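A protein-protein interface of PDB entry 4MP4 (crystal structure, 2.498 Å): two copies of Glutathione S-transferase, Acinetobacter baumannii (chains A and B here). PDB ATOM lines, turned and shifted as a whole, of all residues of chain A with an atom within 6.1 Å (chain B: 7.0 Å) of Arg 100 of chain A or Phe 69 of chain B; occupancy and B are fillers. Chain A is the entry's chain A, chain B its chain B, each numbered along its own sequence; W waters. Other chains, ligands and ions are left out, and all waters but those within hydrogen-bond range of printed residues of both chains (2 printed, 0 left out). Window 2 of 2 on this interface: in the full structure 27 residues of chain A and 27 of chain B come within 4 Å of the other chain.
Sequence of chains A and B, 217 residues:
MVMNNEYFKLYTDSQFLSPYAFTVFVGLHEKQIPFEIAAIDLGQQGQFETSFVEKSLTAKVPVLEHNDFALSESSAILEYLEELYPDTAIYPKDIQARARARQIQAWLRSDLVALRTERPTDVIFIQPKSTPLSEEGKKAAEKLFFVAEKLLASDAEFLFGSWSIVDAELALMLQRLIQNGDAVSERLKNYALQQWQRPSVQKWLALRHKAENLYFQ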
ATOM      1  N   ILE A  95     -10.312 -19.123  28.214  1.00  0.00           N
ATOM      2  CA  ILE A  95      -8.927 -18.709  28.404  1.00  0.00           C
ATOM      3  C   ILE A  95      -8.657 -17.275  27.937  1.00  0.00           C
ATOM      4  O   ILE A  95      -7.847 -16.564  28.543  1.00  0.00           O
ATOM      5  CB  ILE A  95      -7.936 -19.664  27.719  1.00  0.00           C
ATOM      6  CG1 ILE A  95      -6.504 -19.323  28.144  1.00  0.00           C
ATOM      7  CG2 ILE A  95      -8.116 -19.638  26.207  1.00  0.00           C
ATOM      8  CD1 ILE A  95      -5.435 -20.130  27.438  1.00  0.00           C
ATOM      9  N   GLN A  96      -9.344 -16.832  26.889  1.00  0.00           N
ATOM     10  CA  GLN A  96      -9.099 -15.476  26.401  1.00  0.00           C
ATOM     11  C   GLN A  96      -9.810 -14.405  27.225  1.00  0.00           C
ATOM     12  O   GLN A  96      -9.261 -13.330  27.459  1.00  0.00           O
ATOM     13  CB  GLN A  96      -9.358 -15.355  24.900  1.00  0.00           C
ATOM     14  CG  GLN A  96      -8.173 -15.893  24.123  1.00  0.00           C
ATOM     15  CD  GLN A  96      -8.422 -16.086  22.642  1.00  0.00           C
ATOM     16  OE1 GLN A  96      -9.136 -15.311  21.998  1.00  0.00           O
ATOM     17  NE2 GLN A  96      -7.816 -17.131  22.089  1.00  0.00           N
ATOM     18  N   ALA A  97     -11.014 -14.719  27.689  1.00  0.00           N
ATOM     19  CA  ALA A  97     -11.736 -13.829  28.580  1.00  0.00           C
ATOM     20  C   ALA A  97     -10.986 -13.685  29.909  1.00  0.00           C
ATOM     21  O   ALA A  97     -10.896 -12.585  30.447  1.00  0.00           O
ATOM     22  CB  ALA A  97     -13.169 -14.330  28.798  1.00  0.00           C
ATOM     23  N   ARG A  98     -10.432 -14.788  30.417  1.00  0.00           N
ATOM     24  CA  ARG A  98      -9.616 -14.750  31.637  1.00  0.00           C
ATOM     25  C   ARG A  98      -8.372 -13.871  31.490  1.00  0.00           C
ATOM     26  O   ARG A  98      -8.010 -13.120  32.406  1.00  0.00           O
ATOM     27  CB  ARG A  98      -9.199 -16.151  32.073  1.00  0.00           C
ATOM     28  CG  ARG A  98      -8.266 -16.180  33.291  1.00  0.00           C
ATOM     29  CD  ARG A  98      -7.703 -17.574  33.478  1.00  0.00           C
ATOM     30  NE  ARG A  98      -8.780 -18.508  33.219  1.00  0.00           N
ATOM     31  CZ  ARG A  98      -8.741 -19.508  32.353  1.00  0.00           C
ATOM     32  NH1 ARG A  98      -7.639 -19.775  31.665  1.00  0.00           N
ATOM     33  NH2 ARG A  98      -9.819 -20.255  32.211  1.00  0.00           N
ATOM     34  N   ALA A  99      -7.723 -13.971  30.341  1.00  0.00           N
ATOM     35  CA  ALA A  99      -6.574 -13.131  30.043  1.00  0.00           C
ATOM     36  C   ALA A  99      -7.023 -11.672  30.005  1.00  0.00           C
ATOM     37  O   ALA A  99      -6.397 -10.805  30.631  1.00  0.00           O
ATOM     38  CB  ALA A  99      -5.919 -13.547  28.734  1.00  0.00           C
ATOM     39  N   ARG A 100      -8.127 -11.411  29.308  1.00  0.00           N
ATOM     40  CA  ARG A 100      -8.680 -10.057  29.250  1.00  0.00           C
ATOM     41  C   ARG A 100      -9.013  -9.572  30.672  1.00  0.00           C
ATOM     42  O   ARG A 100      -8.692  -8.436  31.046  1.00  0.00           O
ATOM     43  CB  ARG A 100      -9.901  -9.982  28.313  1.00  0.00           C
ATOM     44  CG  ARG A 100     -10.558  -8.591  28.197  1.00  0.00           C
ATOM     45  CD  ARG A 100      -9.801  -7.594  27.268  1.00  0.00           C
ATOM     46  NE  ARG A 100      -9.874  -7.967  25.857  1.00  0.00           N
ATOM     47  CZ  ARG A 100      -8.827  -8.315  25.108  1.00  0.00           C
ATOM     48  NH1 ARG A 100      -8.998  -8.647  23.825  1.00  0.00           N
ATOM     49  NH2 ARG A 100      -7.609  -8.333  25.633  1.00  0.00           N
ATOM     50  N   ALA A 101      -9.621 -10.440  31.475  1.00  0.00           N
ATOM     51  CA  ALA A 101      -9.892 -10.088  32.867  1.00  0.00           C
ATOM     52  C   ALA A 101      -8.613  -9.722  33.647  1.00  0.00           C
ATOM     53  O   ALA A 101      -8.582  -8.711  34.347  1.00  0.00           O
ATOM     54  CB  ALA A 101     -10.678 -11.191  33.579  1.00  0.00           C
ATOM     55  N   ARG A 102      -7.564 -10.531  33.517  1.00  0.00           N
ATOM     56  CA  ARG A 102      -6.283 -10.208  34.154  1.00  0.00           C
ATOM     57  C   ARG A 102      -5.714  -8.900  33.634  1.00  0.00           C
ATOM     58  O   ARG A 102      -5.074  -8.156  34.366  1.00  0.00           O
ATOM     59  CB  ARG A 102      -5.269 -11.335  33.955  1.00  0.00           C
ATOM     60  CG  ARG A 102      -5.567 -12.577  34.794  1.00  0.00           C
ATOM     61  CD  ARG A 102      -4.449 -13.596  34.684  1.00  0.00           C
ATOM     62  NE  ARG A 102      -4.752 -14.807  35.436  1.00  0.00           N
ATOM     63  CZ  ARG A 102      -4.861 -16.018  34.901  1.00  0.00           C
ATOM     64  NH1 ARG A 102      -4.666 -16.200  33.603  1.00  0.00           N
ATOM     65  NH2 ARG A 102      -5.140 -17.054  35.671  1.00  0.00           N
ATOM     66  N   GLN A 103      -5.964  -8.606  32.364  1.00  0.00           N
ATOM     67  CA  GLN A 103      -5.469  -7.370  31.780  1.00  0.00           C
ATOM     68  C   GLN A 103      -6.141  -6.120  32.371  1.00  0.00           C
ATOM     69  O   GLN A 103      -5.463  -5.153  32.751  1.00  0.00           O
ATOM     70  CB  GLN A 103      -5.610  -7.412  30.269  1.00  0.00           C
ATOM     71  CG  GLN A 103      -5.545  -6.065  29.586  1.00  0.00           C
ATOM     72  CD  GLN A 103      -5.999  -6.171  28.138  1.00  0.00           C
ATOM     73  OE1 GLN A 103      -5.784  -7.187  27.495  1.00  0.00           O
ATOM     74  NE2 GLN A 103      -6.643  -5.136  27.634  1.00  0.00           N
ATOM     75  N   ILE A 104      -7.470  -6.149  32.439  1.00  0.00           N
ATOM     76  CA  ILE A 104      -8.242  -5.059  33.026  1.00  0.00           C
ATOM     77  C   ILE A 104      -7.877  -4.848  34.501  1.00  0.00           C
ATOM     78  O   ILE A 104      -7.657  -3.713  34.941  1.00  0.00           O
ATOM     79  CB  ILE A 104      -9.770  -5.280  32.845  1.00  0.00           C
ATOM     80  CG1 ILE A 104     -10.095  -5.432  31.361  1.00  0.00           C
ATOM     81  CG2 ILE A 104     -10.550  -4.134  33.441  1.00  0.00           C
ATOM     82  CD1 ILE A 104      -9.465  -4.301  30.456  1.00  0.00           C
ATOM     83  N   GLN A 105      -7.785  -5.948  35.242  1.00  0.00           N
ATOM     84  CA  GLN A 105      -7.284  -5.942  36.617  1.00  0.00           C
ATOM     85  C   GLN A 105      -5.876  -5.316  36.764  1.00  0.00           C
ATOM     86  O   GLN A 105      -5.633  -4.545  37.697  1.00  0.00           O
ATOM     87  CB  GLN A 105      -7.275  -7.365  37.172  1.00  0.00           C
ATOM     88  CG  GLN A 105      -6.929  -7.457  38.634  1.00  0.00           C
ATOM     89  CD  GLN A 105      -6.992  -8.884  39.147  1.00  0.00           C
ATOM     90  OE1 GLN A 105      -6.138  -9.709  38.827  1.00  0.00           O
ATOM     91  NE2 GLN A 105      -8.006  -9.183  39.941  1.00  0.00           N
ATOM     92  N   LEU A 151     -15.994  -2.529  26.826  1.00  0.00           N
ATOM     93  CA  LEU A 151     -16.170  -3.855  27.403  1.00  0.00           C
ATOM     94  C   LEU A 151     -17.607  -4.129  27.849  1.00  0.00           C
ATOM     95  O   LEU A 151     -17.995  -5.277  28.023  1.00  0.00           O
ATOM     96  CB  LEU A 151     -15.220  -4.051  28.583  1.00  0.00           C
ATOM     97  CG  LEU A 151     -13.718  -4.176  28.311  1.00  0.00           C
ATOM     98  CD1 LEU A 151     -12.979  -4.240  29.628  1.00  0.00           C
ATOM     99  CD2 LEU A 151     -13.400  -5.401  27.460  1.00  0.00           C
ATOM    100  N   PHE A 160     -17.819  -9.990  31.557  1.00  0.00           N
ATOM    101  CA  PHE A 160     -17.411 -11.187  30.836  1.00  0.00           C
ATOM    102  C   PHE A 160     -18.490 -12.271  30.824  1.00  0.00           C
ATOM    103  O   PHE A 160     -18.188 -13.467  30.838  1.00  0.00           O
ATOM    104  CB  PHE A 160     -16.103 -11.728  31.432  1.00  0.00           C
ATOM    105  CG  PHE A 160     -14.985 -10.730  31.411  1.00  0.00           C
ATOM    106  CD1 PHE A 160     -14.443 -10.305  30.204  1.00  0.00           C
ATOM    107  CD2 PHE A 160     -14.498 -10.186  32.589  1.00  0.00           C
ATOM    108  CE1 PHE A 160     -13.425  -9.359  30.170  1.00  0.00           C
ATOM    109  CE2 PHE A 160     -13.481  -9.253  32.564  1.00  0.00           C
ATOM    110  CZ  PHE A 160     -12.941  -8.836  31.350  1.00  0.00           C
ATOM    111  N   TYR B   7       0.790 -18.232  15.314  1.00  0.00           N
ATOM    112  CA  TYR B   7       1.284 -16.873  15.084  1.00  0.00           C
ATOM    113  C   TYR B   7       1.272 -15.986  16.338  1.00  0.00           C
ATOM    114  O   TYR B   7       0.205 -15.719  16.904  1.00  0.00           O
ATOM    115  CB  TYR B   7       0.456 -16.216  13.983  1.00  0.00           C
ATOM    116  CG  TYR B   7       0.666 -14.730  13.810  1.00  0.00           C
ATOM    117  CD1 TYR B   7       1.763 -14.240  13.112  1.00  0.00           C
ATOM    118  CD2 TYR B   7      -0.252 -13.813  14.317  1.00  0.00           C
ATOM    119  CE1 TYR B   7       1.950 -12.875  12.930  1.00  0.00           C
ATOM    120  CE2 TYR B   7      -0.076 -12.454  14.144  1.00  0.00           C
ATOM    121  CZ  TYR B   7       1.030 -11.990  13.447  1.00  0.00           C
ATOM    122  OH  TYR B   7       1.212 -10.637  13.260  1.00  0.00           O
ATOM    123  N   VAL B  63       2.041  -5.171  23.756  1.00  0.00           N
ATOM    124  CA  VAL B  63       0.874  -5.920  23.352  1.00  0.00           C
ATOM    125  C   VAL B  63       1.337  -7.233  22.729  1.00  0.00           C
ATOM    126  O   VAL B  63       2.199  -7.246  21.844  1.00  0.00           O
ATOM    127  CB  VAL B  63      -0.005  -5.127  22.371  1.00  0.00           C
ATOM    128  CG1 VAL B  63      -1.168  -6.012  21.851  1.00  0.00           C
ATOM    129  CG2 VAL B  63      -0.523  -3.857  23.031  1.00  0.00           C
ATOM    130  N   LEU B  64       0.784  -8.340  23.205  1.00  0.00           N
ATOM    131  CA  LEU B  64       0.992  -9.597  22.504  1.00  0.00           C
ATOM    132  C   LEU B  64      -0.192  -9.920  21.591  1.00  0.00           C
ATOM    133  O   LEU B  64      -1.343  -9.943  22.028  1.00  0.00           O
ATOM    134  CB  LEU B  64       1.233 -10.744  23.480  1.00  0.00           C
ATOM    135  CG  LEU B  64       1.623 -12.046  22.772  1.00  0.00           C
ATOM    136  CD1 LEU B  64       2.966 -11.903  22.072  1.00  0.00           C
ATOM    137  CD2 LEU B  64       1.635 -13.227  23.740  1.00  0.00           C
ATOM    138  N   GLU B  65       0.090 -10.166  20.320  1.00  0.00           N
ATOM    139  CA  GLU B  65      -0.949 -10.644  19.421  1.00  0.00           C
ATOM    140  C   GLU B  65      -0.761 -12.129  19.190  1.00  0.00           C
ATOM    141  O   GLU B  65       0.334 -12.583  18.844  1.00  0.00           O
ATOM    142  CB  GLU B  65      -0.989  -9.854  18.112  1.00  0.00           C
ATOM    143  CG  GLU B  65      -1.898  -8.637  18.212  1.00  0.00           C
ATOM    144  CD  GLU B  65      -1.756  -7.657  17.056  1.00  0.00           C
ATOM    145  OE1 GLU B  65      -1.012  -7.961  16.091  1.00  0.00           O
ATOM    146  OE2 GLU B  65      -2.400  -6.576  17.126  1.00  0.00           O
ATOM    147  N   HIS B  66      -1.821 -12.888  19.453  1.00  0.00           N
ATOM    148  CA  HIS B  66      -1.812 -14.321  19.206  1.00  0.00           C
ATOM    149  C   HIS B  66      -2.984 -14.678  18.313  1.00  0.00           C
ATOM    150  O   HIS B  66      -4.125 -14.738  18.779  1.00  0.00           O
ATOM    151  CB  HIS B  66      -1.908 -15.114  20.499  1.00  0.00           C
ATOM    152  CG  HIS B  66      -1.952 -16.594  20.282  1.00  0.00           C
ATOM    153  ND1 HIS B  66      -2.570 -17.460  21.161  1.00  0.00           N
ATOM    154  CD2 HIS B  66      -1.449 -17.364  19.288  1.00  0.00           C
ATOM    155  CE1 HIS B  66      -2.440 -18.697  20.719  1.00  0.00           C
ATOM    156  NE2 HIS B  66      -1.764 -18.667  19.585  1.00  0.00           N
ATOM    157  N   ASN B  67      -2.693 -14.922  17.038  1.00  0.00           N
ATOM    158  CA  ASN B  67      -3.729 -15.105  16.033  1.00  0.00           C
ATOM    159  C   ASN B  67      -4.702 -13.952  16.108  1.00  0.00           C
ATOM    160  O   ASN B  67      -4.327 -12.791  15.960  1.00  0.00           O
ATOM    161  CB  ASN B  67      -4.472 -16.429  16.246  1.00  0.00           C
ATOM    162  CG  ASN B  67      -3.553 -17.632  16.153  1.00  0.00           C
ATOM    163  OD1 ASN B  67      -2.529 -17.588  15.473  1.00  0.00           O
ATOM    164  ND2 ASN B  67      -3.910 -18.708  16.838  1.00  0.00           N
ATOM    165  N   ASP B  68      -5.949 -14.283  16.405  1.00  0.00           N
ATOM    166  CA  ASP B  68      -7.023 -13.305  16.429  1.00  0.00           C
ATOM    167  C   ASP B  68      -7.100 -12.468  17.723  1.00  0.00           C
ATOM    168  O   ASP B  68      -7.866 -11.504  17.811  1.00  0.00           O
ATOM    169  CB  ASP B  68      -8.343 -14.030  16.189  1.00  0.00           C
ATOM    170  CG  ASP B  68      -9.299 -13.211  15.380  1.00  0.00           C
ATOM    171  OD1 ASP B  68      -8.825 -12.252  14.732  1.00  0.00           O
ATOM    172  OD2 ASP B  68     -10.512 -13.518  15.390  1.00  0.00           O
ATOM    173  N   PHE B  69      -6.296 -12.823  18.717  1.00  0.00           N
ATOM    174  CA  PHE B  69      -6.420 -12.236  20.049  1.00  0.00           C
ATOM    175  C   PHE B  69      -5.304 -11.240  20.332  1.00  0.00           C
ATOM    176  O   PHE B  69      -4.136 -11.589  20.244  1.00  0.00           O
ATOM    177  CB  PHE B  69      -6.386 -13.368  21.077  1.00  0.00           C
ATOM    178  CG  PHE B  69      -6.642 -12.933  22.491  1.00  0.00           C
ATOM    179  CD1 PHE B  69      -7.720 -12.125  22.801  1.00  0.00           C
ATOM    180  CD2 PHE B  69      -5.823 -13.368  23.516  1.00  0.00           C
ATOM    181  CE1 PHE B  69      -7.968 -11.744  24.102  1.00  0.00           C
ATOM    182  CE2 PHE B  69      -6.064 -12.993  24.818  1.00  0.00           C
ATOM    183  CZ  PHE B  69      -7.140 -12.184  25.110  1.00  0.00           C
ATOM    184  N   ALA B  70      -5.656 -10.004  20.673  1.00  0.00           N
ATOM    185  CA  ALA B  70      -4.659  -9.031  21.134  1.00  0.00           C
ATOM    186  C   ALA B  70      -4.740  -8.832  22.642  1.00  0.00           C
ATOM    187  O   ALA B  70      -5.831  -8.621  23.187  1.00  0.00           O
ATOM    188  CB  ALA B  70      -4.830  -7.690  20.419  1.00  0.00           C
ATOM    189  N   LEU B  71      -3.588  -8.865  23.312  1.00  0.00           N
ATOM    190  CA  LEU B  71      -3.540  -8.798  24.781  1.00  0.00           C
ATOM    191  C   LEU B  71      -2.441  -7.853  25.298  1.00  0.00           C
ATOM    192  O   LEU B  71      -1.308  -7.868  24.794  1.00  0.00           O
ATOM    193  CB  LEU B  71      -3.354 -10.206  25.362  1.00  0.00           C
ATOM    194  CG  LEU B  71      -3.262 -10.362  26.886  1.00  0.00           C
ATOM    195  CD1 LEU B  71      -4.607 -10.073  27.554  1.00  0.00           C
ATOM    196  CD2 LEU B  71      -2.761 -11.752  27.269  1.00  0.00           C
ATOM    197  N   SER B  72      -2.773  -7.026  26.294  1.00  0.00           N
ATOM    198  CA  SER B  72      -1.779  -6.153  26.919  1.00  0.00           C
ATOM    199  C   SER B  72      -1.611  -6.405  28.428  1.00  0.00           C
ATOM    200  O   SER B  72      -2.309  -7.257  29.004  1.00  0.00           O
ATOM    201  CB  SER B  72      -2.123  -4.686  26.680  1.00  0.00           C
ATOM    202  OG  SER B  72      -3.326  -4.387  27.343  1.00  0.00           O
ATOM    203  N   ALA B  76      -0.418 -10.191  32.739  1.00  0.00           N
ATOM    204  CA  ALA B  76      -1.514 -10.916  32.098  1.00  0.00           C
ATOM    205  C   ALA B  76      -1.001 -11.737  30.919  1.00  0.00           C
ATOM    206  O   ALA B  76      -1.383 -12.896  30.725  1.00  0.00           O
ATOM    207  CB  ALA B  76      -2.623  -9.946  31.655  1.00  0.00           C
ATOM    208  N   TYR B  80      -1.098 -15.839  30.521  1.00  0.00           N
ATOM    209  CA  TYR B  80      -1.682 -16.354  29.287  1.00  0.00           C
ATOM    210  C   TYR B  80      -0.737 -17.361  28.624  1.00  0.00           C
ATOM    211  O   TYR B  80      -1.143 -18.464  28.277  1.00  0.00           O
ATOM    212  CB  TYR B  80      -2.006 -15.184  28.348  1.00  0.00           C
ATOM    213  CG  TYR B  80      -2.603 -15.569  27.024  1.00  0.00           C
ATOM    214  CD1 TYR B  80      -3.805 -16.264  26.952  1.00  0.00           C
ATOM    215  CD2 TYR B  80      -1.983 -15.214  25.837  1.00  0.00           C
ATOM    216  CE1 TYR B  80      -4.354 -16.607  25.746  1.00  0.00           C
ATOM    217  CE2 TYR B  80      -2.526 -15.561  24.619  1.00  0.00           C
ATOM    218  CZ  TYR B  80      -3.712 -16.255  24.578  1.00  0.00           C
ATOM    219  OH  TYR B  80      -4.255 -16.591  23.357  1.00  0.00           O
HETATM  220  O   HOH W   1      -3.882 -14.724  31.244  1.00  0.00           O
HETATM  221  O   HOH W   2      -8.217  -8.945  20.949  1.00  0.00           O
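The guanidinium group of Arg 100 of chain A sits at hydrogen-bond distance from the backbone carbonyl oxygen of Ala 70 of chain B.
The side-chain amide oxygen (OE1) of Gln 103 of chain A lies within hydrogen-bond range of the backbone NH (N) of Ser 72 of chain B (3.2 Å).
OH of Tyr 80 of chain B lies within hydrogen-bond range of ND1 of His 66 of chain B, 2.9 Å away.
O of Leu 71 of chain B is in hydrogen-bond range of N of Leu 64 of chain B, at 2.7 Å.
OE1 of Gln 103 of chain A is in hydrogen-bond range of NH2 of Arg 100 of chain A, 2.8 Å away.
Among the printed residues, merely in contact across the chains: Gln 96 of chain A with Phe 69 of chain B (3.4 Å), Gln 96 of chain A with Tyr 80 of chain B (3.8 Å), Ala 99 of chain A with Phe 69 of chain B (3.96 Å), Ala 99 of chain A with Leu 71 of chain B (3.6 Å), Ala 99 of chain A with Tyr 80 of chain B (3.9 Å), Arg 100 of chain A with Phe 69 of chain B (3.3 Å), Arg 100 of chain A with Leu 71 of chain B (3.97 Å), Arg 102 of chain A with Ala 76 of chain B (3.8 Å), Gln 103 of chain A with Leu 71 of chain B (3.1 Å) and Gln 103 of chain A with Ala 76 of chain B (3.7 Å).
Of the printed residues of chain B, Ala 99 of chain A touches Phe 69, Leu 71 and Tyr 80.
Of the printed residues of chain B, Gln 103 of chain A touches Leu 71, Ser 72 and Ala 76.
His 66 of chain B touches none of the printed residues of chain A.
Phe 69 of chain B touches just these residues of chain A: Gln 96 (3.4 Å), Ala 99 (3.96 Å) and Arg 100 (3.3 Å).
Of the printed residues of chain A, Leu 71 of chain B touches Ala 99 (3.6 Å), Arg 100 (3.97 Å) and Gln 103 (3.1 Å).
Of the printed residues of chain A, Tyr 80 of chain B touches Gln 96 (3.8 Å) and Ala 99 (3.9 Å).
The nearest printed residue of chain A that does not touch Ala 76 of chain B is Ala 99 of chain A (4.004 Å).
Of the 13 printed residues of chain B, 6 touch a printed residue of chain A.
Printed residues of chain B that touch a printed residue of chain A: Phe 69, Ala 70, Leu 71, Ser 72, Ala 76 and Tyr 80.
Hydrophobic or aromatic side chains of chain A within 4 Å of the printed part of chain B: Ala 99.
No position is printed for both chains.
Of the 12 pairs that touch across the chains among the printed residues, none has its exchanged pair printed and touching as well.
Water W2 bridges N of Ala 70 of chain B (2.8 Å) and NH1 of Arg 100 of chain A (3.0 Å).
Water W1 lies within hydrogen-bond range of the guanidinium group of Arg 102 of chain A (2.9 Å), the backbone NH of Tyr 80 of chain B (3.1 Å) and the backbone carbonyl oxygen of Ala 76 of chain B (3.1 Å).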
